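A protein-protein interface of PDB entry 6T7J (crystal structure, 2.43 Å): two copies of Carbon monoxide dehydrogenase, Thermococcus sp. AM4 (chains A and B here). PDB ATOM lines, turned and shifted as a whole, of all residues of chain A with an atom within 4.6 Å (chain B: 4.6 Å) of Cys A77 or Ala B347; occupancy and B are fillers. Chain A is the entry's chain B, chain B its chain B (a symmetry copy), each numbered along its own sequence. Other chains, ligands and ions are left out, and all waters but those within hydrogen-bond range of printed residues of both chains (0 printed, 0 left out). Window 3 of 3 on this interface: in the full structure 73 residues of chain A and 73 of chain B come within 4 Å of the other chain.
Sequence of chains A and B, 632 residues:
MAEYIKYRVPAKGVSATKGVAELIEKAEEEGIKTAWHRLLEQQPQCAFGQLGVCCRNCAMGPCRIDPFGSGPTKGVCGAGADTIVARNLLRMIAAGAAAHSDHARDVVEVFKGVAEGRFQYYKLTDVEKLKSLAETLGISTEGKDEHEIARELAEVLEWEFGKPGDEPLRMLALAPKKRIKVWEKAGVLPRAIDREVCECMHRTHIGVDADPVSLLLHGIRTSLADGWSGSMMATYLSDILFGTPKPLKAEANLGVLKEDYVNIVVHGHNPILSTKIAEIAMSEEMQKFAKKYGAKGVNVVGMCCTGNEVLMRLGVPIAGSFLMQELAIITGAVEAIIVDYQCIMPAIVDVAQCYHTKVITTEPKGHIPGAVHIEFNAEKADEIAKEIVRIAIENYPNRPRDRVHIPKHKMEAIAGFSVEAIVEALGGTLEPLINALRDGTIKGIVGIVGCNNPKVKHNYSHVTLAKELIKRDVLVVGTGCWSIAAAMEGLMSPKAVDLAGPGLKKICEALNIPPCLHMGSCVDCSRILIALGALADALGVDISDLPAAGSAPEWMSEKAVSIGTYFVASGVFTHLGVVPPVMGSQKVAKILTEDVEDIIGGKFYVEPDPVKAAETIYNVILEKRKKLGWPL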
ATOM      1  N   MET A  60     -17.133 -20.662  -1.425  1.00  0.00           N
ATOM      2  CA  MET A  60     -16.870 -19.608  -2.393  1.00  0.00           C
ATOM      3  C   MET A  60     -17.574 -18.307  -2.037  1.00  0.00           C
ATOM      4  O   MET A  60     -17.274 -17.272  -2.639  1.00  0.00           O
ATOM      5  CB  MET A  60     -17.297 -20.057  -3.788  1.00  0.00           C
ATOM      6  CG  MET A  60     -16.790 -21.429  -4.188  1.00  0.00           C
ATOM      7  SD  MET A  60     -16.950 -21.716  -5.959  1.00  0.00           S
ATOM      8  CE  MET A  60     -18.731 -21.784  -6.143  1.00  0.00           C
ATOM      9  N   GLY A  75     -24.344 -14.797  -7.685  1.00  0.00           N
ATOM     10  CA  GLY A  75     -23.296 -15.303  -6.825  1.00  0.00           C
ATOM     11  C   GLY A  75     -22.190 -15.978  -7.619  1.00  0.00           C
ATOM     12  O   GLY A  75     -22.239 -16.106  -8.844  1.00  0.00           O
ATOM     13  N   VAL A  76     -21.160 -16.418  -6.889  1.00  0.00           N
ATOM     14  CA  VAL A  76     -20.012 -17.061  -7.528  1.00  0.00           C
ATOM     15  C   VAL A  76     -20.457 -18.292  -8.312  1.00  0.00           C
ATOM     16  O   VAL A  76     -19.980 -18.546  -9.425  1.00  0.00           O
ATOM     17  CB  VAL A  76     -18.940 -17.410  -6.477  1.00  0.00           C
ATOM     18  CG1 VAL A  76     -17.776 -18.142  -7.122  1.00  0.00           C
ATOM     19  CG2 VAL A  76     -18.443 -16.154  -5.780  1.00  0.00           C
ATOM     20  N   CYS A  77     -21.391 -19.063  -7.750  1.00  0.00           N
ATOM     21  CA  CYS A  77     -21.948 -20.242  -8.403  1.00  0.00           C
ATOM     22  C   CYS A  77     -22.864 -19.899  -9.570  1.00  0.00           C
ATOM     23  O   CYS A  77     -23.183 -20.791 -10.365  1.00  0.00           O
ATOM     24  CB  CYS A  77     -22.729 -21.076  -7.384  1.00  0.00           C
ATOM     25  SG  CYS A  77     -24.301 -20.343  -6.909  1.00  0.00           S
ATOM     26  N   GLY A  78     -23.301 -18.650  -9.682  1.00  0.00           N
ATOM     27  CA  GLY A  78     -24.292 -18.265 -10.661  1.00  0.00           C
ATOM     28  C   GLY A  78     -25.705 -18.155 -10.134  1.00  0.00           C
ATOM     29  O   GLY A  78     -26.623 -17.923 -10.928  1.00  0.00           O
ATOM     30  N   ALA A  79     -25.910 -18.310  -8.826  1.00  0.00           N
ATOM     31  CA  ALA A  79     -27.256 -18.269  -8.267  1.00  0.00           C
ATOM     32  C   ALA A  79     -27.801 -16.849  -8.281  1.00  0.00           C
ATOM     33  O   ALA A  79     -27.169 -15.922  -7.760  1.00  0.00           O
ATOM     34  CB  ALA A  79     -27.269 -18.811  -6.839  1.00  0.00           C
ATOM     35  N   ARG A  87     -33.832 -20.721  -1.289  1.00  0.00           N
ATOM     36  CA  ARG A  87     -33.045 -21.698  -0.541  1.00  0.00           C
ATOM     37  C   ARG A  87     -32.973 -21.340   0.938  1.00  0.00           C
ATOM     38  O   ARG A  87     -33.123 -22.215   1.804  1.00  0.00           O
ATOM     39  CB  ARG A  87     -31.637 -21.805  -1.131  1.00  0.00           C
ATOM     40  CG  ARG A  87     -31.566 -22.540  -2.463  1.00  0.00           C
ATOM     41  CD  ARG A  87     -30.134 -22.922  -2.819  1.00  0.00           C
ATOM     42  NE  ARG A  87     -29.246 -21.763  -2.909  1.00  0.00           N
ATOM     43  CZ  ARG A  87     -28.050 -21.785  -3.490  1.00  0.00           C
ATOM     44  NH1 ARG A  87     -27.597 -22.905  -4.036  1.00  0.00           N
ATOM     45  NH2 ARG A  87     -27.303 -20.689  -3.526  1.00  0.00           N
ATOM     46  N   ILE A 206     -25.081 -26.364  -2.497  1.00  0.00           N
ATOM     47  CA  ILE A 206     -24.649 -25.685  -3.711  1.00  0.00           C
ATOM     48  C   ILE A 206     -24.786 -26.625  -4.900  1.00  0.00           C
ATOM     49  O   ILE A 206     -24.409 -27.802  -4.838  1.00  0.00           O
ATOM     50  CB  ILE A 206     -23.210 -25.163  -3.578  1.00  0.00           C
ATOM     51  CG1 ILE A 206     -22.783 -24.549  -4.911  1.00  0.00           C
ATOM     52  CG2 ILE A 206     -22.248 -26.279  -3.174  1.00  0.00           C
ATOM     53  CD1 ILE A 206     -21.590 -23.669  -4.839  1.00  0.00           C
ATOM     54  N   ARG B  38     -17.209 -13.656 -11.367  1.00  0.00           N
ATOM     55  CA  ARG B  38     -18.215 -13.359 -10.356  1.00  0.00           C
ATOM     56  C   ARG B  38     -17.610 -13.328  -8.957  1.00  0.00           C
ATOM     57  O   ARG B  38     -18.046 -12.534  -8.113  1.00  0.00           O
ATOM     58  CB  ARG B  38     -19.356 -14.371 -10.452  1.00  0.00           C
ATOM     59  CG  ARG B  38     -20.103 -14.297 -11.783  1.00  0.00           C
ATOM     60  CD  ARG B  38     -21.332 -15.185 -11.800  1.00  0.00           C
ATOM     61  NE  ARG B  38     -20.978 -16.596 -11.687  1.00  0.00           N
ATOM     62  CZ  ARG B  38     -20.744 -17.395 -12.724  1.00  0.00           C
ATOM     63  NH1 ARG B  38     -20.831 -16.923 -13.961  1.00  0.00           N
ATOM     64  NH2 ARG B  38     -20.422 -18.665 -12.523  1.00  0.00           N
ATOM     65  N   GLU B 326     -18.125 -24.812 -16.460  1.00  0.00           N
ATOM     66  CA  GLU B 326     -18.369 -23.675 -17.342  1.00  0.00           C
ATOM     67  C   GLU B 326     -17.446 -23.709 -18.549  1.00  0.00           C
ATOM     68  O   GLU B 326     -17.897 -23.621 -19.698  1.00  0.00           O
ATOM     69  CB  GLU B 326     -18.171 -22.366 -16.578  1.00  0.00           C
ATOM     70  CG  GLU B 326     -19.404 -21.827 -15.892  1.00  0.00           C
ATOM     71  CD  GLU B 326     -19.065 -20.686 -14.963  1.00  0.00           C
ATOM     72  OE1 GLU B 326     -17.999 -20.755 -14.313  1.00  0.00           O
ATOM     73  OE2 GLU B 326     -19.851 -19.718 -14.890  1.00  0.00           O
ATOM     74  N   MET B 345     -23.296 -25.926 -11.217  1.00  0.00           N
ATOM     75  CA  MET B 345     -23.402 -24.474 -11.232  1.00  0.00           C
ATOM     76  C   MET B 345     -24.637 -24.061 -12.021  1.00  0.00           C
ATOM     77  O   MET B 345     -24.769 -24.453 -13.188  1.00  0.00           O
ATOM     78  CB  MET B 345     -22.163 -23.842 -11.862  1.00  0.00           C
ATOM     79  CG  MET B 345     -20.900 -23.920 -11.028  1.00  0.00           C
ATOM     80  SD  MET B 345     -19.577 -22.949 -11.782  1.00  0.00           S
ATOM     81  CE  MET B 345     -18.167 -23.460 -10.801  1.00  0.00           C
ATOM     82  N   PRO B 346     -25.565 -23.302 -11.433  1.00  0.00           N
ATOM     83  CA  PRO B 346     -26.667 -22.759 -12.245  1.00  0.00           C
ATOM     84  C   PRO B 346     -26.170 -21.951 -13.429  1.00  0.00           C
ATOM     85  O   PRO B 346     -26.808 -21.948 -14.492  1.00  0.00           O
ATOM     86  CB  PRO B 346     -27.443 -21.890 -11.244  1.00  0.00           C
ATOM     87  CG  PRO B 346     -27.094 -22.456  -9.896  1.00  0.00           C
ATOM     88  CD  PRO B 346     -25.681 -22.941 -10.009  1.00  0.00           C
ATOM     89  N   ALA B 347     -25.012 -21.302 -13.280  1.00  0.00           N
ATOM     90  CA  ALA B 347     -24.454 -20.477 -14.346  1.00  0.00           C
ATOM     91  C   ALA B 347     -24.235 -21.260 -15.634  1.00  0.00           C
ATOM     92  O   ALA B 347     -24.223 -20.664 -16.718  1.00  0.00           O
ATOM     93  CB  ALA B 347     -23.138 -19.851 -13.886  1.00  0.00           C
ATOM     94  N   ILE B 348     -24.060 -22.584 -15.549  1.00  0.00           N
ATOM     95  CA  ILE B 348     -23.839 -23.366 -16.762  1.00  0.00           C
ATOM     96  C   ILE B 348     -25.007 -23.237 -17.725  1.00  0.00           C
ATOM     97  O   ILE B 348     -24.835 -23.450 -18.929  1.00  0.00           O
ATOM     98  CB  ILE B 348     -23.566 -24.856 -16.449  1.00  0.00           C
ATOM     99  CG1 ILE B 348     -24.855 -25.581 -16.052  1.00  0.00           C
ATOM    100  CG2 ILE B 348     -22.477 -25.000 -15.398  1.00  0.00           C
ATOM    101  CD1 ILE B 348     -24.719 -27.084 -16.022  1.00  0.00           C
ATOM    102  N   VAL B 349     -26.196 -22.881 -17.234  1.00  0.00           N
ATOM    103  CA  VAL B 349     -27.293 -22.588 -18.151  1.00  0.00           C
ATOM    104  C   VAL B 349     -27.012 -21.293 -18.902  1.00  0.00           C
ATOM    105  O   VAL B 349     -27.034 -21.259 -20.139  1.00  0.00           O
ATOM    106  CB  VAL B 349     -28.632 -22.534 -17.396  1.00  0.00           C
ATOM    107  CG1 VAL B 349     -29.692 -21.855 -18.246  1.00  0.00           C
ATOM    108  CG2 VAL B 349     -29.072 -23.937 -17.022  1.00  0.00           C
ATOM    109  N   ASP B 350     -26.708 -20.221 -18.164  1.00  0.00           N
ATOM    110  CA  ASP B 350     -26.353 -18.945 -18.780  1.00  0.00           C
ATOM    111  C   ASP B 350     -25.319 -19.130 -19.878  1.00  0.00           C
ATOM    112  O   ASP B 350     -25.553 -18.775 -21.038  1.00  0.00           O
ATOM    113  CB  ASP B 350     -25.823 -17.987 -17.722  1.00  0.00           C
ATOM    114  CG  ASP B 350     -26.916 -17.359 -16.934  1.00  0.00           C
ATOM    115  OD1 ASP B 350     -27.889 -16.830 -17.501  1.00  0.00           O
ATOM    116  OD2 ASP B 350     -26.810 -17.427 -15.717  1.00  0.00           O
ATOM    117  N   VAL B 351     -24.174 -19.719 -19.522  1.00  0.00           N
ATOM    118  CA  VAL B 351     -23.110 -19.963 -20.494  1.00  0.00           C
ATOM    119  C   VAL B 351     -23.650 -20.746 -21.684  1.00  0.00           C
ATOM    120  O   VAL B 351     -23.422 -20.385 -22.847  1.00  0.00           O
ATOM    121  CB  VAL B 351     -21.935 -20.693 -19.820  1.00  0.00           C
ATOM    122  CG1 VAL B 351     -20.843 -21.002 -20.829  1.00  0.00           C
ATOM    123  CG2 VAL B 351     -21.389 -19.860 -18.673  1.00  0.00           C
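NH2 of Arg B38 lies within salt-bridge range of OE2 of Glu B326 (2.7 Å). The backbone NH (N) of Ala A79 sits close to the side-chain sulfur (SG) of Cys A77, 3.2 Å away.
Of the 8 printed residues of chain A, 4 touch a printed residue of chain B. Of the 9 printed residues of chain B, 4 touch a printed residue of chain A. Printed residues of chain B that touch a printed residue of chain A: Arg B38, Met B345, Pro B346 and Ala B347. Hydrophobic or aromatic side chains of chain B that line the printed part of chain A: Met B345, Pro B346 and Ala B347. Among the printed residues, no Asp or Glu carboxylate lies within 4 Å of a Lys or Arg side-chain nitrogen of the other chain.
The backbone carbonyl oxygen (O) of Gly A75 sits at hydrogen-bond distance from the guanidinium group (NE) of Arg B38 (3.1 Å). The backbone carbonyl oxygen (O) of Cys A77 is in hydrogen-bond range of the backbone NH (N) of Ala B347, at 3.5 Å. The backbone carbonyl oxygen of Val A76 sits at hydrogen-bond distance from the guanidinium group of Arg B38, 3.1 Å away.
Among the printed residues, merely in contact across the chains: Cys A77 with Pro B346, Cys A77 with Met B345, Gly A78 with Arg B38 and Gly A78 with Ala B347.
No position is printed for both chains.
Of the printed residues of chain B, Cys A77 touches Met B345, Pro B346 and Ala B347. Ala B347 touches just these residues of chain A: Cys A77 (3.5 Å) and Gly A78 (3.8 Å). Of the printed residues of chain B, Val A76 touches Arg B38 (3.1 Å). Of the printed residues of chain A, Pro B346 touches Cys A77. Printed residues of chain B within 4 Å of Gly A75: Arg B38. Of the printed residues of chain A, Met B345 touches Cys A77 (3.5 Å). Met A60 touches none of the printed residues of chain B. The nearest residue of chain B that does not touch Cys A77 is Arg B38 (4.03 Å).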
